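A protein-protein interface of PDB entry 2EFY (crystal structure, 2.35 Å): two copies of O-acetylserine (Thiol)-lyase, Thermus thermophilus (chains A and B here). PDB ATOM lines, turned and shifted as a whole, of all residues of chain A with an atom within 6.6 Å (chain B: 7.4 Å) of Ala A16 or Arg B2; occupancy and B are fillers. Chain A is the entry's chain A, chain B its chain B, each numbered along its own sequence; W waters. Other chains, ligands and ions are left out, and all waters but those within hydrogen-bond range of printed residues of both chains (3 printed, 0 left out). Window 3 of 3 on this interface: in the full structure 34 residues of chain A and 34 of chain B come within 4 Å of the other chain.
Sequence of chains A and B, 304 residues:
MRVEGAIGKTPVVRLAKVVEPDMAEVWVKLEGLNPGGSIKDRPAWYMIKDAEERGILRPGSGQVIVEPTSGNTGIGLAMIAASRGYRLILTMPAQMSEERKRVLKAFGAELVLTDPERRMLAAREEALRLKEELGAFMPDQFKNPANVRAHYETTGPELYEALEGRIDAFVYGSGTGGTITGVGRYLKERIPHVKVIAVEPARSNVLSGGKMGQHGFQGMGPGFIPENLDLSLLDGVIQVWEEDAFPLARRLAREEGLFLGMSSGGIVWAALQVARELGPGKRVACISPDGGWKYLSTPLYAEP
NZ of Lys A17 lies within hydrogen-bond range of O of Ser B83 (2.9 Å). The backbone NH (N) of Arg A14 lies within hydrogen-bond range of the backbone carbonyl oxygen (O) of Met B1, 2.9 Å away.
The side-chain carboxylate (OE1) of Glu B4 sits at hydrogen-bond distance from the side-chain hydroxyl (OG) of Ser B83. OE1 of Glu A256 is in hydrogen-bond range of N of Lys A17. The backbone NH of Val A18 is in hydrogen-bond range of the side-chain carboxylate of Glu A256 (2.8 Å). The backbone NH (N) of Ala A16 lies within hydrogen-bond range of the side-chain carboxylate (OE2) of Glu A256 (3.1 Å).
CE of Met B1 touches O of Val A12, at 2.8 Å. Met B1 touches Val A13. CG1 of Val A13 touches O of Arg B2, at 3.9 Å. CB of Ala A16 touches NE of Arg B2 (3.5 Å). Glu A256 touches Val B3 (O to CG1, 3.5 Å). Glu A256 touches Ser B83.
Of chain B, only Arg B2 comes within 4 Å of Ala A16. Of the printed residues of chain B, Val A13 touches Met B1 and Arg B2. Of the printed residues of chain B, Glu A256 touches Val B3 (3.5 Å) and Ser B83 (3.7 Å). Of the printed residues of chain B, Arg A14 touches Met B1. Val A19 touches none of the printed residues of chain B. Glu B4 touches none of the printed residues of chain A. The nearest residue of chain B that does not touch Ala A16 is Met B1 (7.1 Å). The nearest printed residue of chain A that does not touch Arg B2 is Lys A17 (4.5 Å).
Hydrophobic or aromatic side chains of chain A within 4 Å of the printed part of chain B: Val A13 and Ala A16. Among the printed residues, 8 pairs touch across the chains.
No position is printed for both chains. Of the 8 pairs that touch across the chains among the printed residues, none has its exchanged pair printed and touching as well.
Water W2 lies within hydrogen-bond range of the backbone NH of Val B3 and the backbone carbonyl oxygen of Glu A256. Water W1 lies within hydrogen-bond range of the side-chain amino group of Lys A17 (3.1 Å) and the backbone carbonyl oxygen of Ser B83 (3.3 Å). Water W3 lies within hydrogen-bond range of the side-chain carboxylate (OE2) of Glu A256 (3.4 Å), the backbone carbonyl oxygen (O) of Ser B83 (3.4 Å) and the side-chain amino group (NZ) of Lys A17 (3.4 Å).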
ATOM      1  N   VAL A  12     -21.533   5.720  17.489  1.00  0.00           N
ATOM      2  CA  VAL A  12     -20.321   5.158  16.938  1.00  0.00           C
ATOM      3  C   VAL A  12     -19.382   6.336  16.712  1.00  0.00           C
ATOM      4  O   VAL A  12     -19.807   7.410  16.287  1.00  0.00           O
ATOM      5  CB  VAL A  12     -20.615   4.412  15.614  1.00  0.00           C
ATOM      6  CG1 VAL A  12     -21.107   5.388  14.560  1.00  0.00           C
ATOM      7  CG2 VAL A  12     -19.372   3.681  15.143  1.00  0.00           C
ATOM      8  N   VAL A  13     -18.111   6.148  17.030  1.00  0.00           N
ATOM      9  CA  VAL A  13     -17.139   7.210  16.854  1.00  0.00           C
ATOM     10  C   VAL A  13     -15.993   6.753  15.981  1.00  0.00           C
ATOM     11  O   VAL A  13     -15.706   5.554  15.887  1.00  0.00           O
ATOM     12  CB  VAL A  13     -16.563   7.675  18.211  1.00  0.00           C
ATOM     13  CG1 VAL A  13     -17.656   8.354  19.032  1.00  0.00           C
ATOM     14  CG2 VAL A  13     -15.969   6.482  18.967  1.00  0.00           C
ATOM     15  N   ARG A  14     -15.335   7.706  15.331  1.00  0.00           N
ATOM     16  CA  ARG A  14     -14.197   7.376  14.485  1.00  0.00           C
ATOM     17  C   ARG A  14     -12.903   7.812  15.156  1.00  0.00           C
ATOM     18  O   ARG A  14     -12.745   8.976  15.514  1.00  0.00           O
ATOM     19  CB  ARG A  14     -14.317   8.049  13.114  1.00  0.00           C
ATOM     20  CG  ARG A  14     -13.089   7.826  12.231  1.00  0.00           C
ATOM     21  CD  ARG A  14     -13.228   8.451  10.842  1.00  0.00           C
ATOM     22  NE  ARG A  14     -11.971   8.356  10.106  1.00  0.00           N
ATOM     23  CZ  ARG A  14     -11.736   8.913   8.919  1.00  0.00           C
ATOM     24  NH1 ARG A  14     -12.679   9.616   8.301  1.00  0.00           N
ATOM     25  NH2 ARG A  14     -10.542   8.774   8.356  1.00  0.00           N
ATOM     26  N   LEU A  15     -11.984   6.869  15.333  1.00  0.00           N
ATOM     27  CA  LEU A  15     -10.697   7.164  15.957  1.00  0.00           C
ATOM     28  C   LEU A  15      -9.919   8.150  15.083  1.00  0.00           C
ATOM     29  O   LEU A  15      -9.918   8.034  13.851  1.00  0.00           O
ATOM     30  CB  LEU A  15      -9.901   5.874  16.135  1.00  0.00           C
ATOM     31  CG  LEU A  15     -10.614   4.797  16.959  1.00  0.00           C
ATOM     32  CD1 LEU A  15      -9.672   3.607  17.142  1.00  0.00           C
ATOM     33  CD2 LEU A  15     -11.034   5.354  18.321  1.00  0.00           C
ATOM     34  N   ALA A  16      -9.252   9.107  15.724  1.00  0.00           N
ATOM     35  CA  ALA A  16      -8.496  10.126  14.998  1.00  0.00           C
ATOM     36  C   ALA A  16      -7.058  10.362  15.464  1.00  0.00           C
ATOM     37  O   ALA A  16      -6.297  11.056  14.789  1.00  0.00           O
ATOM     38  CB  ALA A  16      -9.267  11.453  15.034  1.00  0.00           C
ATOM     39  N   LYS A  17      -6.677   9.802  16.608  1.00  0.00           N
ATOM     40  CA  LYS A  17      -5.316  10.001  17.113  1.00  0.00           C
ATOM     41  C   LYS A  17      -4.513   8.709  17.142  1.00  0.00           C
ATOM     42  O   LYS A  17      -3.347   8.679  16.746  1.00  0.00           O
ATOM     43  CB  LYS A  17      -5.347  10.578  18.527  1.00  0.00           C
ATOM     44  CG  LYS A  17      -6.323  11.713  18.723  1.00  0.00           C
ATOM     45  CD  LYS A  17      -5.839  13.005  18.101  1.00  0.00           C
ATOM     46  CE  LYS A  17      -6.878  14.103  18.316  1.00  0.00           C
ATOM     47  NZ  LYS A  17      -7.287  14.208  19.756  1.00  0.00           N
ATOM     48  N   VAL A  18      -5.139   7.639  17.619  1.00  0.00           N
ATOM     49  CA  VAL A  18      -4.453   6.363  17.708  1.00  0.00           C
ATOM     50  C   VAL A  18      -4.324   5.665  16.367  1.00  0.00           C
ATOM     51  O   VAL A  18      -3.695   4.613  16.272  1.00  0.00           O
ATOM     52  CB  VAL A  18      -5.140   5.423  18.729  1.00  0.00           C
ATOM     53  CG1 VAL A  18      -5.107   6.064  20.099  1.00  0.00           C
ATOM     54  CG2 VAL A  18      -6.561   5.130  18.313  1.00  0.00           C
ATOM     55  N   VAL A  19      -4.920   6.238  15.329  1.00  0.00           N
ATOM     56  CA  VAL A  19      -4.803   5.646  14.001  1.00  0.00           C
ATOM     57  C   VAL A  19      -3.559   6.206  13.337  1.00  0.00           C
ATOM     58  O   VAL A  19      -2.963   7.162  13.832  1.00  0.00           O
ATOM     59  CB  VAL A  19      -6.036   5.939  13.096  1.00  0.00           C
ATOM     60  CG1 VAL A  19      -7.237   5.181  13.619  1.00  0.00           C
ATOM     61  CG2 VAL A  19      -6.327   7.454  13.036  1.00  0.00           C
ATOM     62  N   VAL A  26     -11.341   3.688  11.281  1.00  0.00           N
ATOM     63  CA  VAL A  26     -11.693   2.815  12.389  1.00  0.00           C
ATOM     64  C   VAL A  26     -12.834   3.417  13.192  1.00  0.00           C
ATOM     65  O   VAL A  26     -12.708   4.511  13.741  1.00  0.00           O
ATOM     66  CB  VAL A  26     -10.492   2.538  13.319  1.00  0.00           C
ATOM     67  CG1 VAL A  26     -10.944   1.686  14.485  1.00  0.00           C
ATOM     68  CG2 VAL A  26      -9.381   1.822  12.543  1.00  0.00           C
ATOM     69  N   GLU A 256      -8.212  10.413  22.853  1.00  0.00           N
ATOM     70  CA  GLU A 256      -9.491  10.440  22.153  1.00  0.00           C
ATOM     71  C   GLU A 256     -10.633  10.749  23.104  1.00  0.00           C
ATOM     72  O   GLU A 256     -11.755  11.009  22.675  1.00  0.00           O
ATOM     73  CB  GLU A 256      -9.744   9.090  21.484  1.00  0.00           C
ATOM     74  CG  GLU A 256      -8.550   8.555  20.702  1.00  0.00           C
ATOM     75  CD  GLU A 256      -8.624   8.832  19.201  1.00  0.00           C
ATOM     76  OE1 GLU A 256      -7.737   8.342  18.480  1.00  0.00           O
ATOM     77  OE2 GLU A 256      -9.556   9.527  18.739  1.00  0.00           O
ATOM     78  N   LEU A 258     -11.830   8.633  25.075  1.00  0.00           N
ATOM     79  CA  LEU A 258     -12.611   7.398  25.098  1.00  0.00           C
ATOM     80  C   LEU A 258     -12.134   6.471  26.225  1.00  0.00           C
ATOM     81  O   LEU A 258     -11.170   5.715  26.069  1.00  0.00           O
ATOM     82  CB  LEU A 258     -12.509   6.694  23.741  1.00  0.00           C
ATOM     83  CG  LEU A 258     -13.297   7.384  22.621  1.00  0.00           C
ATOM     84  CD1 LEU A 258     -12.914   6.829  21.270  1.00  0.00           C
ATOM     85  CD2 LEU A 258     -14.785   7.188  22.884  1.00  0.00           C
ATOM     86  N   MET B   1     -17.022  10.930  13.528  1.00  0.00           N
ATOM     87  CA  MET B   1     -17.554  11.616  14.737  1.00  0.00           C
ATOM     88  C   MET B   1     -16.663  11.391  15.960  1.00  0.00           C
ATOM     89  O   MET B   1     -16.259  10.260  16.260  1.00  0.00           O
ATOM     90  CB  MET B   1     -18.980  11.127  15.023  1.00  0.00           C
ATOM     91  CG  MET B   1     -19.589  11.676  16.309  1.00  0.00           C
ATOM     92  SD  MET B   1     -21.368  11.360  16.461  1.00  0.00           S
ATOM     93  CE  MET B   1     -21.388   9.652  17.057  1.00  0.00           C
ATOM     94  N   ARG B   2     -16.348  12.487  16.647  1.00  0.00           N
ATOM     95  CA  ARG B   2     -15.519  12.456  17.855  1.00  0.00           C
ATOM     96  C   ARG B   2     -16.399  12.178  19.073  1.00  0.00           C
ATOM     97  O   ARG B   2     -17.637  12.216  18.983  1.00  0.00           O
ATOM     98  CB  ARG B   2     -14.818  13.798  18.052  1.00  0.00           C
ATOM     99  CG  ARG B   2     -13.936  14.230  16.895  1.00  0.00           C
ATOM    100  CD  ARG B   2     -12.717  13.346  16.763  1.00  0.00           C
ATOM    101  NE  ARG B   2     -11.865  13.775  15.657  1.00  0.00           N
ATOM    102  CZ  ARG B   2     -11.026  14.806  15.705  1.00  0.00           C
ATOM    103  NH1 ARG B   2     -10.913  15.528  16.814  1.00  0.00           N
ATOM    104  NH2 ARG B   2     -10.300  15.114  14.638  1.00  0.00           N
ATOM    105  N   VAL B   3     -15.771  11.918  20.215  1.00  0.00           N
ATOM    106  CA  VAL B   3     -16.534  11.637  21.420  1.00  0.00           C
ATOM    107  C   VAL B   3     -17.542  12.754  21.725  1.00  0.00           C
ATOM    108  O   VAL B   3     -18.710  12.479  22.020  1.00  0.00           O
ATOM    109  CB  VAL B   3     -15.603  11.417  22.642  1.00  0.00           C
ATOM    110  CG1 VAL B   3     -14.823  12.687  22.957  1.00  0.00           C
ATOM    111  CG2 VAL B   3     -16.426  10.969  23.845  1.00  0.00           C
ATOM    112  N   GLU B   4     -17.101  14.008  21.643  1.00  0.00           N
ATOM    113  CA  GLU B   4     -17.985  15.135  21.919  1.00  0.00           C
ATOM    114  C   GLU B   4     -19.235  15.107  21.050  1.00  0.00           C
ATOM    115  O   GLU B   4     -20.254  15.675  21.417  1.00  0.00           O
ATOM    116  CB  GLU B   4     -17.259  16.472  21.715  1.00  0.00           C
ATOM    117  CG  GLU B   4     -16.556  16.600  20.381  1.00  0.00           C
ATOM    118  CD  GLU B   4     -15.090  16.217  20.464  1.00  0.00           C
ATOM    119  OE1 GLU B   4     -14.747  15.334  21.283  1.00  0.00           O
ATOM    120  OE2 GLU B   4     -14.283  16.798  19.704  1.00  0.00           O
ATOM    121  N   GLY B   5     -19.151  14.438  19.903  1.00  0.00           N
ATOM    122  CA  GLY B   5     -20.285  14.348  19.001  1.00  0.00           C
ATOM    123  C   GLY B   5     -21.269  13.268  19.409  1.00  0.00           C
ATOM    124  O   GLY B   5     -22.401  13.235  18.919  1.00  0.00           O
ATOM    125  N   ALA B   6     -20.836  12.380  20.303  1.00  0.00           N
ATOM    126  CA  ALA B   6     -21.681  11.294  20.790  1.00  0.00           C
ATOM    127  C   ALA B   6     -22.431  11.710  22.057  1.00  0.00           C
ATOM    128  O   ALA B   6     -23.062  10.885  22.715  1.00  0.00           O
ATOM    129  CB  ALA B   6     -20.832  10.067  21.072  1.00  0.00           C
ATOM    130  N   ILE B   7     -22.358  12.993  22.395  1.00  0.00           N
ATOM    131  CA  ILE B   7     -23.025  13.524  23.581  1.00  0.00           C
ATOM    132  C   ILE B   7     -24.497  13.857  23.333  1.00  0.00           C
ATOM    133  O   ILE B   7     -24.844  14.413  22.290  1.00  0.00           O
ATOM    134  CB  ILE B   7     -22.328  14.820  24.068  1.00  0.00           C
ATOM    135  CG1 ILE B   7     -20.934  14.501  24.612  1.00  0.00           C
ATOM    136  CG2 ILE B   7     -23.180  15.501  25.125  1.00  0.00           C
ATOM    137  CD1 ILE B   7     -20.141  15.719  25.015  1.00  0.00           C
ATOM    138  N   PRO B  35     -21.507   9.988  27.150  1.00  0.00           N
ATOM    139  CA  PRO B  35     -20.137   9.455  27.125  1.00  0.00           C
ATOM    140  C   PRO B  35     -19.385   9.570  28.455  1.00  0.00           C
ATOM    141  O   PRO B  35     -18.769   8.607  28.908  1.00  0.00           O
ATOM    142  CB  PRO B  35     -19.472  10.274  26.023  1.00  0.00           C
ATOM    143  CG  PRO B  35     -20.597  10.482  25.051  1.00  0.00           C
ATOM    144  CD  PRO B  35     -21.766  10.832  25.965  1.00  0.00           C
ATOM    145  N   PRO B  59      -7.696  23.996  19.486  1.00  0.00           N
ATOM    146  CA  PRO B  59      -7.528  22.560  19.737  1.00  0.00           C
ATOM    147  C   PRO B  59      -6.138  21.998  19.451  1.00  0.00           C
ATOM    148  O   PRO B  59      -5.498  22.356  18.468  1.00  0.00           O
ATOM    149  CB  PRO B  59      -8.639  21.914  18.889  1.00  0.00           C
ATOM    150  CG  PRO B  59      -9.066  22.994  17.927  1.00  0.00           C
ATOM    151  CD  PRO B  59      -8.926  24.258  18.724  1.00  0.00           C
ATOM    152  N   SER B  83     -10.042  14.833  24.468  1.00  0.00           N
ATOM    153  CA  SER B  83     -10.437  14.724  23.068  1.00  0.00           C
ATOM    154  C   SER B  83      -9.877  15.842  22.189  1.00  0.00           C
ATOM    155  O   SER B  83      -9.489  15.611  21.039  1.00  0.00           O
ATOM    156  CB  SER B  83     -11.968  14.728  22.952  1.00  0.00           C
ATOM    157  OG  SER B  83     -12.384  14.600  21.600  1.00  0.00           O
ATOM    158  N   ARG B  84      -9.816  17.047  22.738  1.00  0.00           N
ATOM    159  CA  ARG B  84      -9.356  18.184  21.967  1.00  0.00           C
ATOM    160  C   ARG B  84      -7.940  18.658  22.244  1.00  0.00           C
ATOM    161  O   ARG B  84      -7.549  19.741  21.819  1.00  0.00           O
ATOM    162  CB  ARG B  84     -10.360  19.322  22.135  1.00  0.00           C
ATOM    163  CG  ARG B  84     -11.785  18.867  21.771  1.00  0.00           C
ATOM    164  CD  ARG B  84     -12.773  20.007  21.746  1.00  0.00           C
ATOM    165  NE  ARG B  84     -12.569  20.922  20.624  1.00  0.00           N
ATOM    166  CZ  ARG B  84     -12.747  20.604  19.343  1.00  0.00           C
ATOM    167  NH1 ARG B  84     -13.132  19.380  18.998  1.00  0.00           N
ATOM    168  NH2 ARG B  84     -12.560  21.523  18.404  1.00  0.00           N
HETATM  169  O   HOH W   1      -7.461  17.251  18.992  1.00  0.00           O
HETATM  170  O   HOH W   2     -13.057  11.200  20.166  1.00  0.00           O
HETATM  171  O   HOH W   3     -10.384  12.763  19.356  1.00  0.00           O
